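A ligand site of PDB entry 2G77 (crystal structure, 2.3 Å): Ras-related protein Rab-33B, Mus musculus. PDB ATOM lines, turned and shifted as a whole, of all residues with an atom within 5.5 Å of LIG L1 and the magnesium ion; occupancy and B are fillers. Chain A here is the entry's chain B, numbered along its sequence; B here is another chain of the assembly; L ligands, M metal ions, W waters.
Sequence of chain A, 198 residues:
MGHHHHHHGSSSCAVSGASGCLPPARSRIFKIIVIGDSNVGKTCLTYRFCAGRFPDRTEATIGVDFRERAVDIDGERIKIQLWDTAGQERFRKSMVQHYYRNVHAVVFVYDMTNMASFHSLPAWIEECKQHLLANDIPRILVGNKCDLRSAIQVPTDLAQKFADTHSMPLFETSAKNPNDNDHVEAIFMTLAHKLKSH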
ATOM      1  N   ASP A  37       5.843  -0.431  11.806  1.00  0.00           N
ATOM      2  CA  ASP A  37       4.519  -0.107  11.275  1.00  0.00           C
ATOM      3  C   ASP A  37       3.407  -0.403  12.240  1.00  0.00           C
ATOM      4  O   ASP A  37       3.582  -1.165  13.198  1.00  0.00           O
ATOM      5  CB  ASP A  37       4.250  -0.798   9.924  1.00  0.00           C
ATOM      6  CG  ASP A  37       5.018  -0.135   8.772  1.00  0.00           C
ATOM      7  OD1 ASP A  37       5.874   0.753   9.095  1.00  0.00           O
ATOM      8  OD2 ASP A  37       4.817  -0.528   7.592  1.00  0.00           O
ATOM      9  N   SER A  38       2.285   0.301  12.071  1.00  0.00           N
ATOM     10  CA  SER A  38       1.054  -0.017  12.806  1.00  0.00           C
ATOM     11  C   SER A  38       0.720  -1.559  12.710  1.00  0.00           C
ATOM     12  O   SER A  38       0.815  -2.123  11.623  1.00  0.00           O
ATOM     13  CB  SER A  38      -0.095   0.798  12.164  1.00  0.00           C
ATOM     14  OG  SER A  38      -1.338   0.448  12.759  1.00  0.00           O
ATOM     15  N   ASN A  39       0.340  -2.209  13.803  1.00  0.00           N
ATOM     16  CA  ASN A  39      -0.258  -3.552  13.765  1.00  0.00           C
ATOM     17  C   ASN A  39       0.721  -4.712  13.657  1.00  0.00           C
ATOM     18  O   ASN A  39       0.284  -5.861  13.536  1.00  0.00           O
ATOM     19  CB  ASN A  39      -1.358  -3.675  12.670  1.00  0.00           C
ATOM     20  CG  ASN A  39      -2.409  -4.752  13.018  1.00  0.00           C
ATOM     21  OD1 ASN A  39      -3.057  -4.707  14.050  1.00  0.00           O
ATOM     22  ND2 ASN A  39      -2.573  -5.705  12.123  1.00  0.00           N
ATOM     23  N   VAL A  40       2.007  -4.439  13.757  1.00  0.00           N
ATOM     24  CA  VAL A  40       3.026  -5.488  13.590  1.00  0.00           C
ATOM     25  C   VAL A  40       3.201  -6.209  14.943  1.00  0.00           C
ATOM     26  O   VAL A  40       3.710  -7.325  14.998  1.00  0.00           O
ATOM     27  CB  VAL A  40       4.382  -4.927  13.083  1.00  0.00           C
ATOM     28  CG1 VAL A  40       4.260  -4.201  11.706  1.00  0.00           C
ATOM     29  CG2 VAL A  40       5.079  -4.093  14.187  1.00  0.00           C
ATOM     30  N   GLY A  41       2.773  -5.560  16.040  1.00  0.00           N
ATOM     31  CA  GLY A  41       2.745  -6.185  17.338  1.00  0.00           C
ATOM     32  C   GLY A  41       3.704  -5.565  18.299  1.00  0.00           C
ATOM     33  O   GLY A  41       4.130  -6.233  19.218  1.00  0.00           O
ATOM     34  N   LYS A  42       4.028  -4.292  18.144  1.00  0.00           N
ATOM     35  CA  LYS A  42       4.967  -3.665  19.084  1.00  0.00           C
ATOM     36  C   LYS A  42       4.423  -3.742  20.513  1.00  0.00           C
ATOM     37  O   LYS A  42       5.182  -4.079  21.463  1.00  0.00           O
ATOM     38  CB  LYS A  42       5.346  -2.222  18.688  1.00  0.00           C
ATOM     39  CG  LYS A  42       5.757  -2.055  17.229  1.00  0.00           C
ATOM     40  CD  LYS A  42       6.013  -0.578  16.898  1.00  0.00           C
ATOM     41  CE  LYS A  42       4.675   0.253  16.738  1.00  0.00           C
ATOM     42  NZ  LYS A  42       3.796  -0.443  15.752  1.00  0.00           N
ATOM     43  N   THR A  43       3.114  -3.518  20.701  1.00  0.00           N
ATOM     44  CA  THR A  43       2.589  -3.447  22.086  1.00  0.00           C
ATOM     45  C   THR A  43       2.570  -4.819  22.675  1.00  0.00           C
ATOM     46  O   THR A  43       2.898  -4.973  23.825  1.00  0.00           O
ATOM     47  CB  THR A  43       1.172  -2.801  22.142  1.00  0.00           C
ATOM     48  OG1 THR A  43       1.281  -1.445  21.764  1.00  0.00           O
ATOM     49  CG2 THR A  43       0.569  -2.821  23.514  1.00  0.00           C
ATOM     50  N   CYS A  44       2.123  -5.829  21.914  1.00  0.00           N
ATOM     51  CA  CYS A  44       2.210  -7.222  22.387  1.00  0.00           C
ATOM     52  C   CYS A  44       3.649  -7.674  22.745  1.00  0.00           C
ATOM     53  O   CYS A  44       3.884  -8.251  23.802  1.00  0.00           O
ATOM     54  CB  CYS A  44       1.623  -8.198  21.383  1.00  0.00           C
ATOM     55  SG  CYS A  44      -0.146  -7.953  21.088  1.00  0.00           S
ATOM     56  N   LEU A  45       4.604  -7.378  21.885  1.00  0.00           N
ATOM     57  CA  LEU A  45       6.023  -7.683  22.164  1.00  0.00           C
ATOM     58  C   LEU A  45       6.515  -7.021  23.441  1.00  0.00           C
ATOM     59  O   LEU A  45       7.143  -7.661  24.274  1.00  0.00           O
ATOM     60  CB  LEU A  45       6.926  -7.193  21.017  1.00  0.00           C
ATOM     61  CG  LEU A  45       7.950  -8.084  20.348  1.00  0.00           C
ATOM     62  CD1 LEU A  45       9.202  -7.207  19.925  1.00  0.00           C
ATOM     63  CD2 LEU A  45       8.361  -9.323  21.136  1.00  0.00           C
ATOM     64  N   PHE A  54       1.045 -12.111  26.994  1.00  0.00           N
ATOM     65  CA  PHE A  54       0.514 -11.602  25.752  1.00  0.00           C
ATOM     66  C   PHE A  54      -0.846 -10.914  25.983  1.00  0.00           C
ATOM     67  O   PHE A  54      -1.783 -11.589  26.402  1.00  0.00           O
ATOM     68  CB  PHE A  54       0.296 -12.731  24.760  1.00  0.00           C
ATOM     69  CG  PHE A  54      -0.264 -12.277  23.423  1.00  0.00           C
ATOM     70  CD1 PHE A  54       0.535 -11.593  22.501  1.00  0.00           C
ATOM     71  CD2 PHE A  54      -1.583 -12.556  23.084  1.00  0.00           C
ATOM     72  CE1 PHE A  54       0.037 -11.210  21.271  1.00  0.00           C
ATOM     73  CE2 PHE A  54      -2.101 -12.148  21.856  1.00  0.00           C
ATOM     74  CZ  PHE A  54      -1.266 -11.467  20.948  1.00  0.00           C
ATOM     75  N   PRO A  55      -0.971  -9.595  25.667  1.00  0.00           N
ATOM     76  CA  PRO A  55      -2.225  -8.845  25.900  1.00  0.00           C
ATOM     77  C   PRO A  55      -3.148  -9.166  24.739  1.00  0.00           C
ATOM     78  O   PRO A  55      -2.889  -8.755  23.592  1.00  0.00           O
ATOM     79  CB  PRO A  55      -1.752  -7.382  25.864  1.00  0.00           C
ATOM     80  CG  PRO A  55      -0.681  -7.403  24.881  1.00  0.00           C
ATOM     81  CD  PRO A  55       0.046  -8.733  25.023  1.00  0.00           C
ATOM     82  N   ASP A  56      -4.186  -9.928  24.989  1.00  0.00           N
ATOM     83  CA  ASP A  56      -5.008 -10.299  23.840  1.00  0.00           C
ATOM     84  C   ASP A  56      -6.074  -9.250  23.430  1.00  0.00           C
ATOM     85  O   ASP A  56      -6.789  -9.456  22.474  1.00  0.00           O
ATOM     86  CB  ASP A  56      -5.648 -11.655  24.030  1.00  0.00           C
ATOM     87  CG  ASP A  56      -6.755 -11.617  25.043  1.00  0.00           C
ATOM     88  OD1 ASP A  56      -6.614 -10.837  26.049  1.00  0.00           O
ATOM     89  OD2 ASP A  56      -7.748 -12.355  24.813  1.00  0.00           O
ATOM     90  N   THR A  58      -5.373  -5.496  22.792  1.00  0.00           N
ATOM     91  CA  THR A  58      -4.690  -4.184  22.711  1.00  0.00           C
ATOM     92  C   THR A  58      -5.599  -3.116  22.076  1.00  0.00           C
ATOM     93  O   THR A  58      -6.584  -3.432  21.379  1.00  0.00           O
ATOM     94  CB  THR A  58      -3.355  -4.253  21.921  1.00  0.00           C
ATOM     95  OG1 THR A  58      -3.573  -4.804  20.620  1.00  0.00           O
ATOM     96  CG2 THR A  58      -2.362  -5.118  22.661  1.00  0.00           C
ATOM     97  N   GLU A  59      -5.281  -1.861  22.366  1.00  0.00           N
ATOM     98  CA  GLU A  59      -5.860  -0.741  21.682  1.00  0.00           C
ATOM     99  C   GLU A  59      -4.798  -0.239  20.686  1.00  0.00           C
ATOM    100  O   GLU A  59      -3.636  -0.574  20.821  1.00  0.00           O
ATOM    101  CB  GLU A  59      -6.251   0.341  22.695  1.00  0.00           C
ATOM    102  CG  GLU A  59      -7.564  -0.025  23.454  1.00  0.00           C
ATOM    103  CD  GLU A  59      -7.980   1.075  24.416  1.00  0.00           C
ATOM    104  OE1 GLU A  59      -7.340   1.174  25.468  1.00  0.00           O
ATOM    105  OE2 GLU A  59      -8.933   1.866  24.116  1.00  0.00           O
ATOM    106  N   ALA A  60      -5.184   0.555  19.701  1.00  0.00           N
ATOM    107  CA  ALA A  60      -4.195   1.143  18.824  1.00  0.00           C
ATOM    108  C   ALA A  60      -3.454   2.112  19.761  1.00  0.00           C
ATOM    109  O   ALA A  60      -4.098   2.881  20.490  1.00  0.00           O
ATOM    110  CB  ALA A  60      -4.865   1.852  17.683  1.00  0.00           C
ATOM    111  N   THR A  61      -2.134   2.001  19.849  1.00  0.00           N
ATOM    112  CA  THR A  61      -1.326   2.894  20.699  1.00  0.00           C
ATOM    113  C   THR A  61      -1.348   4.295  20.111  1.00  0.00           C
ATOM    114  O   THR A  61      -1.207   4.474  18.872  1.00  0.00           O
ATOM    115  CB  THR A  61       0.170   2.391  20.799  1.00  0.00           C
ATOM    116  OG1 THR A  61       0.167   1.009  21.234  1.00  0.00           O
ATOM    117  CG2 THR A  61       1.066   3.304  21.671  1.00  0.00           C
ATOM    118  N   ASP A  84       7.054   2.204  23.748  1.00  0.00           N
ATOM    119  CA  ASP A  84       6.337   1.549  22.683  1.00  0.00           C
ATOM    120  C   ASP A  84       5.598   2.603  21.819  1.00  0.00           C
ATOM    121  O   ASP A  84       4.631   3.216  22.282  1.00  0.00           O
ATOM    122  CB  ASP A  84       5.374   0.520  23.293  1.00  0.00           C
ATOM    123  CG  ASP A  84       4.360   0.083  22.358  1.00  0.00           C
ATOM    124  OD1 ASP A  84       4.672   0.103  21.119  1.00  0.00           O
ATOM    125  OD2 ASP A  84       3.221  -0.273  22.831  1.00  0.00           O
ATOM    126  N   THR A  85       6.052   2.825  20.568  1.00  0.00           N
ATOM    127  CA  THR A  85       5.485   3.913  19.778  1.00  0.00           C
ATOM    128  C   THR A  85       4.233   3.550  18.973  1.00  0.00           C
ATOM    129  O   THR A  85       3.992   2.354  18.681  1.00  0.00           O
ATOM    130  CB  THR A  85       6.479   4.511  18.740  1.00  0.00           C
ATOM    131  OG1 THR A  85       6.833   3.496  17.766  1.00  0.00           O
ATOM    132  CG2 THR A  85       7.734   5.035  19.440  1.00  0.00           C
ATOM    133  N   ASN A 144       7.927 -10.629  13.706  1.00  0.00           N
ATOM    134  CA  ASN A 144       6.953 -11.078  14.690  1.00  0.00           C
ATOM    135  C   ASN A 144       5.845 -11.862  14.012  1.00  0.00           C
ATOM    136  O   ASN A 144       5.755 -11.906  12.771  1.00  0.00           O
ATOM    137  CB  ASN A 144       6.393  -9.881  15.521  1.00  0.00           C
ATOM    138  CG  ASN A 144       5.440 -10.339  16.679  1.00  0.00           C
ATOM    139  OD1 ASN A 144       5.667 -11.399  17.276  1.00  0.00           O
ATOM    140  ND2 ASN A 144       4.385  -9.569  16.967  1.00  0.00           N
ATOM    141  N   LYS A 145       5.007 -12.476  14.808  1.00  0.00           N
ATOM    142  CA  LYS A 145       3.880 -13.239  14.254  1.00  0.00           C
ATOM    143  C   LYS A 145       4.287 -14.512  13.465  1.00  0.00           C
ATOM    144  O   LYS A 145       3.593 -14.950  12.522  1.00  0.00           O
ATOM    145  CB  LYS A 145       2.982 -12.339  13.356  1.00  0.00           C
ATOM    146  CG  LYS A 145       2.423 -11.054  14.080  1.00  0.00           C
ATOM    147  CD  LYS A 145       1.241 -10.454  13.336  1.00  0.00           C
ATOM    148  CE  LYS A 145       0.708  -9.182  13.989  1.00  0.00           C
ATOM    149  NZ  LYS A 145      -0.258  -8.412  13.102  1.00  0.00           N
ATOM    150  N   CYS A 146       5.390 -15.128  13.841  1.00  0.00           N
ATOM    151  CA  CYS A 146       5.774 -16.331  13.083  1.00  0.00           C
ATOM    152  C   CYS A 146       4.867 -17.563  13.286  1.00  0.00           C
ATOM    153  O   CYS A 146       4.890 -18.514  12.503  1.00  0.00           O
ATOM    154  CB  CYS A 146       7.201 -16.677  13.355  1.00  0.00           C
ATOM    155  SG  CYS A 146       7.238 -17.594  14.783  1.00  0.00           S
ATOM    156  N   ASP A 147       4.084 -17.480  14.198  1.00  0.00           N
ATOM    157  CA  ASP A 147       2.972 -18.427  14.246  1.00  0.00           C
ATOM    158  C   ASP A 147       1.988 -18.351  13.075  1.00  0.00           C
ATOM    159  O   ASP A 147       1.281 -19.307  12.797  1.00  0.00           O
ATOM    160  CB  ASP A 147       2.240 -18.335  15.583  1.00  0.00           C
ATOM    161  CG  ASP A 147       1.611 -16.980  15.822  1.00  0.00           C
ATOM    162  OD1 ASP A 147       2.354 -15.983  15.775  1.00  0.00           O
ATOM    163  OD2 ASP A 147       0.404 -16.822  16.080  1.00  0.00           O
ATOM    164  N   LEU A 148       1.914 -17.279  12.344  1.00  0.00           N
ATOM    165  CA  LEU A 148       1.068 -17.405  11.184  1.00  0.00           C
ATOM    166  C   LEU A 148       1.773 -18.111  10.024  1.00  0.00           C
ATOM    167  O   LEU A 148       2.079 -17.481   9.022  1.00  0.00           O
ATOM    168  CB  LEU A 148       0.420 -16.080  10.834  1.00  0.00           C
ATOM    169  CG  LEU A 148      -0.305 -15.473  12.046  1.00  0.00           C
ATOM    170  CD1 LEU A 148      -0.686 -14.034  11.836  1.00  0.00           C
ATOM    171  CD2 LEU A 148      -1.509 -16.299  12.432  1.00  0.00           C
ATOM    172  N   THR A 173      10.142 -14.453  15.594  1.00  0.00           N
ATOM    173  CA  THR A 173       9.424 -14.959  16.779  1.00  0.00           C
ATOM    174  C   THR A 173       7.917 -14.715  16.746  1.00  0.00           C
ATOM    175  O   THR A 173       7.357 -14.286  15.711  1.00  0.00           O
ATOM    176  CB  THR A 173      10.053 -14.398  18.073  1.00  0.00           C
ATOM    177  OG1 THR A 173       9.709 -15.239  19.178  1.00  0.00           O
ATOM    178  CG2 THR A 173       9.612 -12.918  18.374  1.00  0.00           C
ATOM    179  N   SER A 174       7.259 -15.047  17.813  1.00  0.00           N
ATOM    180  CA  SER A 174       5.852 -14.790  18.048  1.00  0.00           C
ATOM    181  C   SER A 174       5.657 -14.270  19.453  1.00  0.00           C
ATOM    182  O   SER A 174       5.977 -14.950  20.420  1.00  0.00           O
ATOM    183  CB  SER A 174       5.021 -16.060  17.825  1.00  0.00           C
ATOM    184  OG  SER A 174       3.644 -15.785  17.698  1.00  0.00           O
ATOM    185  N   ALA A 175       5.107 -13.078  19.560  1.00  0.00           N
ATOM    186  CA  ALA A 175       4.603 -12.541  20.875  1.00  0.00           C
ATOM    187  C   ALA A 175       3.363 -13.300  21.391  1.00  0.00           C
ATOM    188  O   ALA A 175       3.145 -13.362  22.581  1.00  0.00           O
ATOM    189  CB  ALA A 175       4.308 -11.036  20.807  1.00  0.00           C
ATOM    190  N   LYS A 176       2.586 -13.890  20.494  1.00  0.00           N
ATOM    191  CA  LYS A 176       1.390 -14.583  20.873  1.00  0.00           C
ATOM    192  C   LYS A 176       1.577 -16.075  21.248  1.00  0.00           C
ATOM    193  O   LYS A 176       1.026 -16.463  22.286  1.00  0.00           O
ATOM    194  CB  LYS A 176       0.367 -14.511  19.779  1.00  0.00           C
ATOM    195  CG  LYS A 176      -0.954 -15.174  20.139  1.00  0.00           C
ATOM    196  CD  LYS A 176      -1.955 -15.086  18.969  1.00  0.00           C
ATOM    197  CE  LYS A 176      -3.373 -15.439  19.475  1.00  0.00           C
ATOM    198  NZ  LYS A 176      -4.475 -14.845  18.626  1.00  0.00           N
ATOM    199  N   ASN A 177       2.277 -16.866  20.399  1.00  0.00           N
ATOM    200  CA  ASN A 177       2.558 -18.291  20.642  1.00  0.00           C
ATOM    201  C   ASN A 177       3.116 -18.524  22.057  1.00  0.00           C
ATOM    202  O   ASN A 177       4.184 -17.995  22.413  1.00  0.00           O
ATOM    203  CB  ASN A 177       3.533 -18.895  19.609  1.00  0.00           C
ATOM    204  CG  ASN A 177       3.407 -20.453  19.481  1.00  0.00           C
ATOM    205  OD1 ASN A 177       2.990 -21.151  20.420  1.00  0.00           O
ATOM    206  ND2 ASN A 177       3.767 -20.971  18.308  1.00  0.00           N
ATOM    207  N   ARG B 116      -9.556  -3.219  17.373  1.00  0.00           N
ATOM    208  CA  ARG B 116      -8.790  -2.790  18.546  1.00  0.00           C
ATOM    209  C   ARG B 116      -9.430  -1.565  19.190  1.00  0.00           C
ATOM    210  O   ARG B 116      -8.777  -0.889  19.997  1.00  0.00           O
ATOM    211  CB  ARG B 116      -7.364  -2.464  18.180  1.00  0.00           C
ATOM    212  CG  ARG B 116      -6.456  -3.682  17.800  1.00  0.00           C
ATOM    213  CD  ARG B 116      -4.965  -3.234  17.665  1.00  0.00           C
ATOM    214  NE  ARG B 116      -4.826  -2.420  16.452  1.00  0.00           N
ATOM    215  CZ  ARG B 116      -3.693  -1.781  16.119  1.00  0.00           C
ATOM    216  NH1 ARG B 116      -2.628  -1.856  16.900  1.00  0.00           N
ATOM    217  NH2 ARG B 116      -3.640  -1.022  15.021  1.00  0.00           N
HETATM  218  P1  LIG L   1       1.071  -2.457  17.274  1.00  0.00           P
HETATM  219  O1  LIG L   1       0.282  -1.441  16.449  1.00  0.00           O
HETATM  220  O2  LIG L   1       2.413  -2.625  16.661  1.00  0.00           O
HETATM  221  O3  LIG L   1       1.176  -2.225  18.722  1.00  0.00           O
HETATM  222  O4  LIG L   1       0.200  -3.821  17.143  1.00  0.00           O
HETATM  223  P2  LIG L   1      -0.404  -4.567  18.410  1.00  0.00           P
HETATM  224  O5  LIG L   1      -1.527  -3.780  19.030  1.00  0.00           O
HETATM  225  O6  LIG L   1       0.545  -4.916  19.520  1.00  0.00           O
HETATM  226  O7  LIG L   1      -0.979  -5.897  17.744  1.00  0.00           O
HETATM  227  C1  LIG L   1      -1.776  -5.764  16.562  1.00  0.00           C
HETATM  228  C2  LIG L   1      -2.525  -7.072  16.259  1.00  0.00           C
HETATM  229  O8  LIG L   1      -1.600  -8.181  16.001  1.00  0.00           O
HETATM  230  C3  LIG L   1      -3.314  -7.455  17.508  1.00  0.00           C
HETATM  231  O9  LIG L   1      -4.547  -8.078  17.099  1.00  0.00           O
HETATM  232  C4  LIG L   1      -2.454  -8.491  18.205  1.00  0.00           C
HETATM  233  O10 LIG L   1      -3.242  -9.464  18.894  1.00  0.00           O
HETATM  234  C5  LIG L   1      -1.767  -9.170  17.038  1.00  0.00           C
HETATM  235  N1  LIG L   1      -0.464  -9.778  17.365  1.00  0.00           N
HETATM  236  C6  LIG L   1       0.571  -9.267  17.989  1.00  0.00           C
HETATM  237  N2  LIG L   1       1.574 -10.190  18.067  1.00  0.00           N
HETATM  238  C7  LIG L   1       1.154 -11.339  17.489  1.00  0.00           C
HETATM  239  C8  LIG L   1       1.704 -12.700  17.200  1.00  0.00           C
HETATM  240  O11 LIG L   1       2.886 -13.046  17.519  1.00  0.00           O
HETATM  241  N3  LIG L   1       0.927 -13.555  16.564  1.00  0.00           N
HETATM  242  C9  LIG L   1      -0.310 -13.267  16.179  1.00  0.00           C
HETATM  243  N4  LIG L   1      -0.996 -14.218  15.516  1.00  0.00           N
HETATM  244  N5  LIG L   1      -0.878 -12.032  16.373  1.00  0.00           N
HETATM  245  C10 LIG L   1      -0.190 -11.043  17.023  1.00  0.00           C
HETATM  246 AL1  LG2 L   2       0.081   0.897  16.748  1.00  0.00          AL
HETATM  247  F1  LG2 L   2      -0.337   0.889  18.346  1.00  0.00           F
HETATM  248  F2  LG2 L   2       1.653   1.328  16.293  1.00  0.00           F
HETATM  249  F3  LG2 L   2      -1.046   0.477  15.610  1.00  0.00           F
HETATM  250 MG    MG M   1       0.722  -0.529  20.017  1.00  0.00          MG
HETATM  251  O   HOH W   1      -6.528  -7.519  19.243  1.00  0.00           O
HETATM  252  O   HOH W   2      -6.809  -7.032  15.738  1.00  0.00           O
HETATM  253  O   HOH W   3       2.506   0.368  19.807  1.00  0.00           O
HETATM  254  O   HOH W   4      -4.423 -11.843  18.342  1.00  0.00           O
HETATM  255  O   HOH W   5      -1.111  -1.547  20.253  1.00  0.00           O
HETATM  256  O   HOH W   6      -4.053  -8.068  21.018  1.00  0.00           O
HETATM  257  O   HOH W   7      -2.567 -10.718  13.791  1.00  0.00           O
HETATM  258  O   HOH W   8      -3.852 -13.929  15.084  1.00  0.00           O
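N of Thr 43 lies within hydrogen-bond range of O6 of LIG L1, 3.2 Å away.
N of Lys 42 lies within hydrogen-bond range of O2 of LIG L1, 2.8 Å away.
The side-chain amino group (NZ) of Lys 42 lies within salt-bridge range of an oxygen (O2) of LIG L1, 2.7 Å away.
The backbone NH of Asn 39 sits close to an oxygen (O1) of LIG L1, 2.8 Å away.
O5 of LIG L1 sits at hydrogen-bond distance from OG1 of Thr 58, at 2.8 Å.
The side-chain hydroxyl (OG) of Ser 174 sits at hydrogen-bond distance from an oxygen (O11) of LIG L1, 2.8 Å away.
The side-chain carboxylate of Asp 147 lies within hydrogen-bond range of a nitrogen (N3) of LIG L1, at 2.9 Å.
The guanidinium group (NH1) of Arg 116 of chain B is in salt-bridge range of an oxygen (O5) of LIG L1 (3.1 Å).
N of Cys 44 is in hydrogen-bond range of O6 of LIG L1, at 3.0 Å.
An oxygen (O6) of LIG L1 sits close to the side-chain sulfur (SG) of Cys 44.
The backbone NH (N) of Ala 175 lies within hydrogen-bond range of an oxygen (O11) of LIG L1 (3.0 Å).
N of Gly 41 is in hydrogen-bond range of O2 of LIG L1, 3.0 Å away.
N2 of LIG L1 sits at hydrogen-bond distance from ND2 of Asn 144 (3.1 Å).
N of Lys 176 sits at hydrogen-bond distance from O11 of LIG L1 (3.1 Å).
The backbone NH (N) of Lys 145 lies close to an oxygen (O11) of LIG L1, 3.5 Å away.
An oxygen (O8) of LIG L1 lies within hydrogen-bond range of the side-chain amino group of Lys 145 (3.2 Å).
An oxygen (O2) of LIG L1 sits at hydrogen-bond distance from the backbone NH of Val 40 (3.4 Å).
N of Thr 61 lies close to F1 of LG2 L2 (2.6 Å).
A fluorine (F2) of LG2 L2 sits at hydrogen-bond distance from the side-chain amino group (NZ) of Lys 42 (2.8 Å).
NH2 of Arg 116 of chain B sits at hydrogen-bond distance from F3 of LG2 L2, at 3.1 Å.
OG of Ser 38 is in hydrogen-bond range of F3 of LG2 L2, at 2.9 Å.
An aluminium atom (AL1) of LG2 L2 is bound by an oxygen (O1) of LIG L1 (2.4 Å).
The side-chain hydroxyl of Thr 43 lies close to the side-chain carboxylate of Asp 84 (2.5 Å).
NZ of Lys 42 lies within hydrogen-bond range of O of Asp 37.
The side-chain amino group (NZ) of Lys 145 is in hydrogen-bond range of the backbone carbonyl oxygen (O) of Asn 39 (2.6 Å).
The backbone NH (N) of Asn 177 lies within hydrogen-bond range of the side-chain hydroxyl (OG) of Ser 174, 3.2 Å away.
SG of Cys 44 lies within hydrogen-bond range of O of Pro 55 (3.8 Å).
N of Ala 175 sits at hydrogen-bond distance from OD1 of Asn 144 (2.9 Å).
The side-chain amide nitrogen (ND2) of Asn 144 is in hydrogen-bond range of the backbone carbonyl oxygen (O) of Val 40 (3.1 Å).
The backbone NH (N) of Lys 145 is in hydrogen-bond range of the backbone carbonyl oxygen (O) of Thr 173, at 3.1 Å.
Residues that only touch LIG L1: Phe 54, Leu 148, Ser 38 and Asp 37.
Hydrophobic or aromatic side chains within 4 Å of LIG L1: Val 40, Phe 54, Leu 148 and Ala 175.
Within 4 Å of LIG L1: Asp 37, Ser 38, Asn 39, Val 40, Gly 41, Lys 42, Thr 43, Cys 44, Phe 54, Thr 58, Asn 144, Lys 145, Asp 147, Leu 148, Ser 174, Ala 175, Lys 176 and Arg 116 of chain B.
Merely in contact with the magnesium ion: Asp 84 (3.8 Å).
Three residues have an atom within 4 Å of the magnesium ion: Thr 43, Thr 61 and Asp 84.
The nearest printed residue that does not touch the magnesium ion is Glu 59 (4.4 Å).
The magnesium ion is bound by water W3 (2.0 Å).
The magnesium ion is bound by the side-chain hydroxyl (OG1) of Thr 61 (2.0 Å).
The magnesium ion is bound by the side-chain hydroxyl (OG1) of Thr 43.
The magnesium ion is bound by water W5.
O3 of LIG L1 is bound to the magnesium ion, 2.2 Å away.
F1 of LG2 L2 is bound to the magnesium ion (2.4 Å).
Water W3 lies within hydrogen-bond range of OD1 of Asp 84 (2.5 Å) and O of Thr 85 (2.7 Å).
Water W5 bridges an oxygen (O5) of LIG L1 and the backbone carbonyl oxygen (O) of Glu 59.
Water W6 lies within hydrogen-bond range of an oxygen (O10) of LIG L1 (2.7 Å), the backbone carbonyl oxygen of Pro 55 (2.9 Å), the side-chain hydroxyl of Thr 58 (3.3 Å) and the backbone carbonyl oxygen of Asp 56 (3.4 Å).
Water W4 bridges O10 of LIG L1 (2.7 Å) and NZ of Lys 176 (3.0 Å).
Water W7 lies within hydrogen-bond range of NZ of Lys 145 (3.3 Å) and N5 of LIG L1 (3.4 Å).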
